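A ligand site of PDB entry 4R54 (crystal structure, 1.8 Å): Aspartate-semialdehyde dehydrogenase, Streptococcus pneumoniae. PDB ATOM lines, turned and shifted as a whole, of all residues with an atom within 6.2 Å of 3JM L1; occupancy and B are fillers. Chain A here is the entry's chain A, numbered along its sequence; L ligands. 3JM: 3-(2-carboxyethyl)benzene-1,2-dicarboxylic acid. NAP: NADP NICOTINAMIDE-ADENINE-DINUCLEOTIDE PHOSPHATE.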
ATOM      1  N   ALA A  72      14.812 -16.205 -29.688  1.00  0.00           N
ATOM      2  CA  ALA A  72      15.742 -16.950 -28.863  1.00  0.00           C
ATOM      3  C   ALA A  72      15.301 -17.037 -27.411  1.00  0.00           C
ATOM      4  O   ALA A  72      16.117 -17.301 -26.520  1.00  0.00           O
ATOM      5  CB  ALA A  72      17.123 -16.307 -28.946  1.00  0.00           C
ATOM      6  N   GLY A  73      14.011 -16.806 -27.172  1.00  0.00           N
ATOM      7  CA  GLY A  73      13.430 -16.924 -25.841  1.00  0.00           C
ATOM      8  C   GLY A  73      13.250 -15.568 -25.193  1.00  0.00           C
ATOM      9  O   GLY A  73      13.986 -14.631 -25.506  1.00  0.00           O
ATOM     10  N   SER A  74      12.275 -15.479 -24.295  1.00  0.00           N
ATOM     11  CA  SER A  74      11.897 -14.227 -23.628  1.00  0.00           C
ATOM     12  C   SER A  74      13.041 -13.561 -22.904  1.00  0.00           C
ATOM     13  O   SER A  74      13.210 -12.348 -22.996  1.00  0.00           O
ATOM     14  CB  SER A  74      10.770 -14.486 -22.622  1.00  0.00           C
ATOM     15  OG  SER A  74       9.536 -14.552 -23.314  1.00  0.00           O
ATOM     16  N   SER A  75      13.813 -14.372 -22.167  1.00  0.00           N
ATOM     17  CA  SER A  75      14.977 -13.889 -21.445  1.00  0.00           C
ATOM     18  C   SER A  75      15.962 -13.163 -22.363  1.00  0.00           C
ATOM     19  O   SER A  75      16.387 -12.052 -22.067  1.00  0.00           O
ATOM     20  CB  SER A  75      15.660 -15.051 -20.743  1.00  0.00           C
ATOM     21  OG  SER A  75      16.894 -14.658 -20.174  1.00  0.00           O
ATOM     22  N   THR A  76      16.318 -13.807 -23.481  1.00  0.00           N
ATOM     23  CA  THR A  76      17.214 -13.201 -24.465  1.00  0.00           C
ATOM     24  C   THR A  76      16.639 -11.880 -25.030  1.00  0.00           C
ATOM     25  O   THR A  76      17.363 -10.899 -25.165  1.00  0.00           O
ATOM     26  CB  THR A  76      17.538 -14.214 -25.592  1.00  0.00           C
ATOM     27  OG1 THR A  76      18.198 -15.356 -25.030  1.00  0.00           O
ATOM     28  CG2 THR A  76      18.443 -13.612 -26.647  1.00  0.00           C
ATOM     29  N   ASN A  94       9.822 -12.109 -31.574  1.00  0.00           N
ATOM     30  CA  ASN A  94       8.930 -13.233 -31.661  1.00  0.00           C
ATOM     31  C   ASN A  94       8.532 -13.833 -30.310  1.00  0.00           C
ATOM     32  O   ASN A  94       7.753 -14.785 -30.274  1.00  0.00           O
ATOM     33  CB  ASN A  94       9.564 -14.289 -32.556  1.00  0.00           C
ATOM     34  CG  ASN A  94       8.561 -15.274 -33.071  1.00  0.00           C
ATOM     35  OD1 ASN A  94       7.472 -14.891 -33.509  1.00  0.00           O
ATOM     36  ND2 ASN A  94       8.896 -16.563 -33.013  1.00  0.00           N
ATOM     37  N   THR A  95       9.007 -13.283 -29.203  1.00  0.00           N
ATOM     38  CA  THR A  95       8.710 -13.825 -27.883  1.00  0.00           C
ATOM     39  C   THR A  95       7.539 -13.125 -27.236  1.00  0.00           C
ATOM     40  O   THR A  95       7.072 -12.094 -27.729  1.00  0.00           O
ATOM     41  CB  THR A  95       9.891 -13.691 -26.915  1.00  0.00           C
ATOM     42  OG1 THR A  95       9.977 -12.334 -26.425  1.00  0.00           O
ATOM     43  CG2 THR A  95      11.154 -14.094 -27.605  1.00  0.00           C
ATOM     44  N   SER A  96       7.120 -13.629 -26.079  1.00  0.00           N
ATOM     45  CA  SER A  96       6.020 -13.034 -25.333  1.00  0.00           C
ATOM     46  C   SER A  96       6.401 -11.774 -24.554  1.00  0.00           C
ATOM     47  O   SER A  96       5.513 -11.058 -24.090  1.00  0.00           O
ATOM     48  CB  SER A  96       5.435 -14.055 -24.346  1.00  0.00           C
ATOM     49  OG  SER A  96       6.430 -14.473 -23.403  1.00  0.00           O
ATOM     50  N   TYR A  97       7.698 -11.504 -24.397  1.00  0.00           N
ATOM     51  CA  TYR A  97       8.148 -10.577 -23.371  1.00  0.00           C
ATOM     52  C   TYR A  97       7.572  -9.168 -23.445  1.00  0.00           C
ATOM     53  O   TYR A  97       7.109  -8.633 -22.444  1.00  0.00           O
ATOM     54  CB  TYR A  97       9.682 -10.517 -23.313  1.00  0.00           C
ATOM     55  CG  TYR A  97      10.172  -9.825 -22.067  1.00  0.00           C
ATOM     56  CD1 TYR A  97      10.178 -10.482 -20.838  1.00  0.00           C
ATOM     57  CD2 TYR A  97      10.571  -8.490 -22.111  1.00  0.00           C
ATOM     58  CE1 TYR A  97      10.593  -9.826 -19.686  1.00  0.00           C
ATOM     59  CE2 TYR A  97      10.979  -7.827 -20.969  1.00  0.00           C
ATOM     60  CZ  TYR A  97      10.991  -8.506 -19.760  1.00  0.00           C
ATOM     61  OH  TYR A  97      11.404  -7.837 -18.639  1.00  0.00           O
ATOM     62  N   ARG A  99       5.002  -8.143 -25.449  1.00  0.00           N
ATOM     63  CA  ARG A  99       3.692  -8.120 -26.144  1.00  0.00           C
ATOM     64  C   ARG A  99       2.639  -7.231 -25.499  1.00  0.00           C
ATOM     65  O   ARG A  99       1.787  -6.691 -26.205  1.00  0.00           O
ATOM     66  CB  ARG A  99       3.143  -9.526 -26.289  1.00  0.00           C
ATOM     67  CG  ARG A  99       3.941 -10.402 -27.239  1.00  0.00           C
ATOM     68  CD  ARG A  99       3.262 -11.722 -27.417  1.00  0.00           C
ATOM     69  NE  ARG A  99       3.962 -12.579 -28.359  1.00  0.00           N
ATOM     70  CZ  ARG A  99       4.080 -13.901 -28.230  1.00  0.00           C
ATOM     71  NH1 ARG A  99       3.516 -14.515 -27.200  1.00  0.00           N
ATOM     72  NH2 ARG A  99       4.762 -14.594 -29.132  1.00  0.00           N
ATOM     73  N   CYS A 125       5.690  -9.898 -32.452  1.00  0.00           N
ATOM     74  CA  CYS A 125       4.919 -10.913 -33.149  1.00  0.00           C
ATOM     75  C   CYS A 125       4.114 -11.681 -32.058  1.00  0.00           C
ATOM     76  O   CYS A 125       4.675 -12.066 -31.023  1.00  0.00           O
ATOM     77  CB  CYS A 125       5.881 -11.785 -33.984  1.00  0.00           C
ATOM     78  SG  CYS A 125       5.222 -13.254 -34.778  1.00  0.00           S
ATOM     79  N   PRO A 126       2.789 -11.839 -32.242  1.00  0.00           N
ATOM     80  CA  PRO A 126       1.995 -12.561 -31.231  1.00  0.00           C
ATOM     81  C   PRO A 126       2.317 -14.043 -31.206  1.00  0.00           C
ATOM     82  O   PRO A 126       3.050 -14.542 -32.063  1.00  0.00           O
ATOM     83  CB  PRO A 126       0.536 -12.338 -31.661  1.00  0.00           C
ATOM     84  CG  PRO A 126       0.574 -11.305 -32.744  1.00  0.00           C
ATOM     85  CD  PRO A 126       1.947 -11.309 -33.336  1.00  0.00           C
ATOM     86  N   ASN A 127       1.762 -14.730 -30.229  1.00  0.00           N
ATOM     87  CA  ASN A 127       1.788 -16.192 -30.159  1.00  0.00           C
ATOM     88  C   ASN A 127       1.133 -16.846 -31.381  1.00  0.00           C
ATOM     89  O   ASN A 127       0.119 -16.343 -31.882  1.00  0.00           O
ATOM     90  CB  ASN A 127       1.067 -16.615 -28.872  1.00  0.00           C
ATOM     91  CG  ASN A 127       0.883 -18.098 -28.789  1.00  0.00           C
ATOM     92  OD1 ASN A 127      -0.190 -18.613 -29.070  1.00  0.00           O
ATOM     93  ND2 ASN A 127       1.951 -18.818 -28.441  1.00  0.00           N
ATOM     94  N   CYS A 128       1.703 -17.968 -31.835  1.00  0.00           N
ATOM     95  CA  CYS A 128       1.240 -18.684 -33.028  1.00  0.00           C
ATOM     96  C   CYS A 128      -0.247 -18.952 -33.034  1.00  0.00           C
ATOM     97  O   CYS A 128      -0.960 -18.676 -34.029  1.00  0.00           O
ATOM     98  CB  CYS A 128       2.031 -19.998 -33.203  1.00  0.00           C
ATOM     99  SG  CYS A 128       2.354 -20.899 -31.666  1.00  0.00           S
ATOM    100  N   GLY A 159       6.281 -26.132 -31.818  1.00  0.00           N
ATOM    101  CA  GLY A 159       6.046 -24.928 -31.062  1.00  0.00           C
ATOM    102  C   GLY A 159       6.847 -24.842 -29.783  1.00  0.00           C
ATOM    103  O   GLY A 159       7.090 -23.755 -29.288  1.00  0.00           O
ATOM    104  N   ALA A 160       7.290 -25.985 -29.263  1.00  0.00           N
ATOM    105  CA  ALA A 160       8.123 -26.015 -28.073  1.00  0.00           C
ATOM    106  C   ALA A 160       9.608 -26.243 -28.373  1.00  0.00           C
ATOM    107  O   ALA A 160      10.370 -26.485 -27.447  1.00  0.00           O
ATOM    108  CB  ALA A 160       7.594 -27.053 -27.061  1.00  0.00           C
ATOM    109  N   ASP A 210       2.928 -24.100 -21.766  1.00  0.00           N
ATOM    110  CA  ASP A 210       3.546 -23.123 -20.862  1.00  0.00           C
ATOM    111  C   ASP A 210       3.191 -23.456 -19.412  1.00  0.00           C
ATOM    112  O   ASP A 210       2.602 -24.488 -19.126  1.00  0.00           O
ATOM    113  CB  ASP A 210       3.136 -21.688 -21.221  1.00  0.00           C
ATOM    114  CG  ASP A 210       4.278 -20.687 -21.078  1.00  0.00           C
ATOM    115  OD1 ASP A 210       4.893 -20.559 -19.988  1.00  0.00           O
ATOM    116  OD2 ASP A 210       4.566 -19.988 -22.068  1.00  0.00           O
ATOM    117  N   GLU A 220      -0.192 -19.933 -21.816  1.00  0.00           N
ATOM    118  CA  GLU A 220      -0.534 -20.012 -23.240  1.00  0.00           C
ATOM    119  C   GLU A 220      -2.005 -19.610 -23.444  1.00  0.00           C
ATOM    120  O   GLU A 220      -2.324 -18.856 -24.363  1.00  0.00           O
ATOM    121  CB  GLU A 220      -0.301 -21.439 -23.774  1.00  0.00           C
ATOM    122  CG  GLU A 220      -0.653 -21.670 -25.248  1.00  0.00           C
ATOM    123  CD  GLU A 220       0.206 -20.888 -26.242  1.00  0.00           C
ATOM    124  OE1 GLU A 220       1.175 -20.241 -25.805  1.00  0.00           O
ATOM    125  OE2 GLU A 220      -0.071 -20.934 -27.465  1.00  0.00           O
ATOM    126  N   LYS A 223      -2.242 -15.798 -22.811  1.00  0.00           N
ATOM    127  CA  LYS A 223      -1.719 -15.085 -23.967  1.00  0.00           C
ATOM    128  C   LYS A 223      -2.795 -14.980 -25.047  1.00  0.00           C
ATOM    129  O   LYS A 223      -2.988 -13.915 -25.594  1.00  0.00           O
ATOM    130  CB  LYS A 223      -0.470 -15.737 -24.534  1.00  0.00           C
ATOM    131  CG  LYS A 223       0.760 -15.599 -23.662  1.00  0.00           C
ATOM    132  CD  LYS A 223       1.984 -16.140 -24.410  1.00  0.00           C
ATOM    133  CE  LYS A 223       2.863 -17.057 -23.594  1.00  0.00           C
ATOM    134  NZ  LYS A 223       3.325 -18.174 -24.463  1.00  0.00           N
ATOM    135  N   GLU A 227      -3.764 -11.272 -25.929  1.00  0.00           N
ATOM    136  CA  GLU A 227      -3.250 -10.856 -27.217  1.00  0.00           C
ATOM    137  C   GLU A 227      -4.409 -10.527 -28.160  1.00  0.00           C
ATOM    138  O   GLU A 227      -4.347  -9.526 -28.888  1.00  0.00           O
ATOM    139  CB  GLU A 227      -2.285 -11.892 -27.787  1.00  0.00           C
ATOM    140  CG  GLU A 227      -0.992 -11.959 -26.955  1.00  0.00           C
ATOM    141  CD  GLU A 227      -0.065 -13.116 -27.339  1.00  0.00           C
ATOM    142  OE1 GLU A 227      -0.228 -13.669 -28.443  1.00  0.00           O
ATOM    143  OE2 GLU A 227       0.853 -13.465 -26.533  1.00  0.00           O
ATOM    144  N   ARG A 245      -1.321 -29.811 -26.198  1.00  0.00           N
ATOM    145  CA  ARG A 245      -0.331 -30.415 -27.064  1.00  0.00           C
ATOM    146  C   ARG A 245      -0.735 -31.810 -27.528  1.00  0.00           C
ATOM    147  O   ARG A 245      -1.154 -32.628 -26.713  1.00  0.00           O
ATOM    148  CB  ARG A 245       1.011 -30.541 -26.318  1.00  0.00           C
ATOM    149  CG  ARG A 245       2.193 -30.745 -27.261  1.00  0.00           C
ATOM    150  CD  ARG A 245       2.582 -29.463 -27.977  1.00  0.00           C
ATOM    151  NE  ARG A 245       3.135 -28.474 -27.063  1.00  0.00           N
ATOM    152  CZ  ARG A 245       3.464 -27.225 -27.390  1.00  0.00           C
ATOM    153  NH1 ARG A 245       3.351 -26.786 -28.642  1.00  0.00           N
ATOM    154  NH2 ARG A 245       3.936 -26.415 -26.456  1.00  0.00           N
HETATM  155  C7  3JM L   1       6.064 -20.023 -27.408  1.00  0.00           C
HETATM  156  O19 3JM L   1      11.850 -17.858 -23.246  1.00  0.00           O
HETATM  157  C15 3JM L   1      10.911 -18.664 -23.152  1.00  0.00           C
HETATM  158  O16 3JM L   1      10.894 -19.633 -22.368  1.00  0.00           O
HETATM  159  C14 3JM L   1       9.738 -18.420 -24.066  1.00  0.00           C
HETATM  160  C13 3JM L   1       8.915 -19.694 -24.223  1.00  0.00           C
HETATM  161  C4  3JM L   1       7.899 -19.723 -25.346  1.00  0.00           C
HETATM  162  C3  3JM L   1       7.123 -18.614 -25.757  1.00  0.00           C
HETATM  163  C10 3JM L   1       7.290 -17.253 -25.117  1.00  0.00           C
HETATM  164  O12 3JM L   1       7.983 -16.394 -25.699  1.00  0.00           O
HETATM  165  O11 3JM L   1       6.788 -16.984 -24.014  1.00  0.00           O
HETATM  166  C5  3JM L   1       7.728 -20.962 -25.954  1.00  0.00           C
HETATM  167  C6  3JM L   1       6.817 -21.119 -26.990  1.00  0.00           C
HETATM  168  C2  3JM L   1       6.207 -18.772 -26.809  1.00  0.00           C
HETATM  169  C1  3JM L   1       5.325 -17.656 -27.324  1.00  0.00           C
HETATM  170  O8  3JM L   1       5.311 -17.402 -28.532  1.00  0.00           O
HETATM  171  O9  3JM L   1       4.570 -17.021 -26.552  1.00  0.00           O
HETATM  172  PA  NAP L   2      14.625 -23.805 -30.015  1.00  0.00           P
HETATM  173  O1A NAP L   2      14.982 -24.468 -28.705  1.00  0.00           O
HETATM  174  O2A NAP L   2      14.426 -24.635 -31.237  1.00  0.00           O
HETATM  175  O5B NAP L   2      15.771 -22.704 -30.295  1.00  0.00           O
HETATM  176  C5B NAP L   2      16.239 -21.841 -29.284  1.00  0.00           C
HETATM  177  C4B NAP L   2      17.069 -20.756 -29.981  1.00  0.00           C
HETATM  178  O4B NAP L   2      17.397 -19.724 -29.053  1.00  0.00           O
HETATM  179  C3B NAP L   2      18.393 -21.290 -30.501  1.00  0.00           C
HETATM  180  O3B NAP L   2      18.772 -20.575 -31.663  1.00  0.00           O
HETATM  181  C2B NAP L   2      19.353 -20.978 -29.375  1.00  0.00           C
HETATM  182  O2B NAP L   2      20.723 -20.895 -29.757  1.00  0.00           O
HETATM  183  C1B NAP L   2      18.809 -19.644 -28.936  1.00  0.00           C
HETATM  184  N9A NAP L   2      19.238 -19.296 -27.570  1.00  0.00           N
HETATM  185  C8A NAP L   2      19.008 -19.964 -26.425  1.00  0.00           C
HETATM  186  N7A NAP L   2      19.591 -19.294 -25.387  1.00  0.00           N
HETATM  187  C5A NAP L   2      20.187 -18.207 -25.887  1.00  0.00           C
HETATM  188  C6A NAP L   2      20.983 -17.087 -25.364  1.00  0.00           C
HETATM  189  N6A NAP L   2      21.252 -16.987 -24.049  1.00  0.00           N
HETATM  190  N1A NAP L   2      21.412 -16.151 -26.232  1.00  0.00           N
HETATM  191  C2A NAP L   2      21.152 -16.222 -27.544  1.00  0.00           C
HETATM  192  N3A NAP L   2      20.452 -17.206 -28.096  1.00  0.00           N
HETATM  193  C4A NAP L   2      19.949 -18.205 -27.321  1.00  0.00           C
HETATM  194  O3  NAP L   2      13.335 -22.868 -29.818  1.00  0.00           O
HETATM  195  PN  NAP L   2      12.391 -22.261 -31.003  1.00  0.00           P
HETATM  196  O1N NAP L   2      11.196 -23.160 -31.231  1.00  0.00           O
HETATM  197  O2N NAP L   2      13.162 -21.804 -32.217  1.00  0.00           O
HETATM  198  O5D NAP L   2      11.844 -20.954 -30.269  1.00  0.00           O
HETATM  199  C5D NAP L   2      12.682 -20.118 -29.487  1.00  0.00           C
HETATM  200  C4D NAP L   2      11.833 -18.967 -28.976  1.00  0.00           C
HETATM  201  O4D NAP L   2      11.091 -18.326 -30.037  1.00  0.00           O
HETATM  202  C3D NAP L   2      10.781 -19.428 -27.977  1.00  0.00           C
HETATM  203  O3D NAP L   2      11.311 -19.668 -26.684  1.00  0.00           O
HETATM  204  C2D NAP L   2       9.768 -18.305 -28.081  1.00  0.00           C
HETATM  205  O2D NAP L   2      10.115 -17.178 -27.270  1.00  0.00           O
HETATM  206  C1D NAP L   2       9.814 -17.913 -29.550  1.00  0.00           C
HETATM  207  N1N NAP L   2       8.716 -18.584 -30.253  1.00  0.00           N
HETATM  208  C2N NAP L   2       7.585 -17.925 -30.521  1.00  0.00           C
HETATM  209  C3N NAP L   2       6.539 -18.551 -31.196  1.00  0.00           C
HETATM  210  C7N NAP L   2       5.244 -17.858 -31.514  1.00  0.00           C
HETATM  211  O7N NAP L   2       4.207 -18.438 -31.229  1.00  0.00           O
HETATM  212  N7N NAP L   2       5.228 -16.653 -32.081  1.00  0.00           N
HETATM  213  C4N NAP L   2       6.660 -19.890 -31.574  1.00  0.00           C
HETATM  214  C5N NAP L   2       7.823 -20.553 -31.274  1.00  0.00           C
HETATM  215  C6N NAP L   2       8.839 -19.886 -30.610  1.00  0.00           C
HETATM  216  P2B NAP L   2      21.735 -22.109 -29.458  1.00  0.00           P
HETATM  217  O1X NAP L   2      21.487 -23.049 -30.602  1.00  0.00           O
HETATM  218  O2X NAP L   2      23.110 -21.468 -29.447  1.00  0.00           O
HETATM  219  O3X NAP L   2      21.308 -22.691 -28.153  1.00  0.00           O
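Gly 73 touches 3JM L1 (CA to O19, 3.2 Å). Asn 94 touches 3JM L1 (O to O8, 3.98 Å). Thr 95 touches 3JM L1 (CA to O12, 3.4 Å). Asn 127 touches 3JM L1 (ND2 to O8, 3.6 Å). Gly 159 touches 3JM L1 (O to C6, 3.5 Å). Within 4 Å of 3JM L1: Gly 73, Ser 74, Asn 94, Thr 95, Ser 96, Arg 99, Asn 127, Gly 159 and Lys 223. Along chain A the residues within 4 Å of 3JM L1 span positions 73 to 223. The nearest printed residue that does not touch 3JM L1 is Ser 75 (4.1 Å).
NZ of Lys 223 is in salt-bridge range of O9 of 3JM L1, 2.7 Å away. OG of Ser 96 is in hydrogen-bond range of O11 of 3JM L1 (2.6 Å). An oxygen (O7N) of NAP L2 is in hydrogen-bond range of the side-chain sulfur (SG) of Cys 128. NH1 of Arg 99 lies within salt-bridge range of O9 of 3JM L1, 2.8 Å away. The backbone NH (N) of Ser 96 lies within hydrogen-bond range of an oxygen (O12) of 3JM L1. The backbone carbonyl oxygen of Pro 126 is in hydrogen-bond range of a nitrogen (N7N) of NAP L2 (3.0 Å). An oxygen (O19) of 3JM L1 lies within hydrogen-bond range of the backbone NH (N) of Ser 74, at 2.6 Å. The backbone NH (N) of Cys 128 sits at hydrogen-bond distance from an oxygen (O7N) of NAP L2. OG of Ser 74 sits at hydrogen-bond distance from O12 of 3JM L1, 3.4 Å away. OD1 of Asn 94 is in hydrogen-bond range of N7N of NAP L2 (3.2 Å).
The guanidinium group (NH2) of Arg 99 is in hydrogen-bond range of the backbone carbonyl oxygen (O) of Asn 94, at 3.2 Å. The guanidinium group (NE) of Arg 99 sits at hydrogen-bond distance from the backbone carbonyl oxygen (O) of Cys 125. The backbone carbonyl oxygen (O) of Thr 95 lies within hydrogen-bond range of the guanidinium group (NE) of Arg 99 (3.2 Å). OD1 of Asn 127 sits close to OE2 of Glu 220 (2.8 Å). The backbone NH (N) of Asn 127 lies within hydrogen-bond range of the side-chain carboxylate (OE1) of Glu 227, 2.9 Å away. The guanidinium group (NH1) of Arg 99 is in salt-bridge range of the side-chain carboxylate (OE2) of Glu 227 (2.9 Å). The side-chain hydroxyl (OG) of Ser 96 sits at hydrogen-bond distance from the side-chain hydroxyl (OG) of Ser 74, 3.1 Å away. NZ of Lys 223 is in salt-bridge range of OE1 of Glu 220, 3.3 Å away.
An oxygen (O12) of 3JM L1 is in hydrogen-bond range of an oxygen (O2D) of NAP L2.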
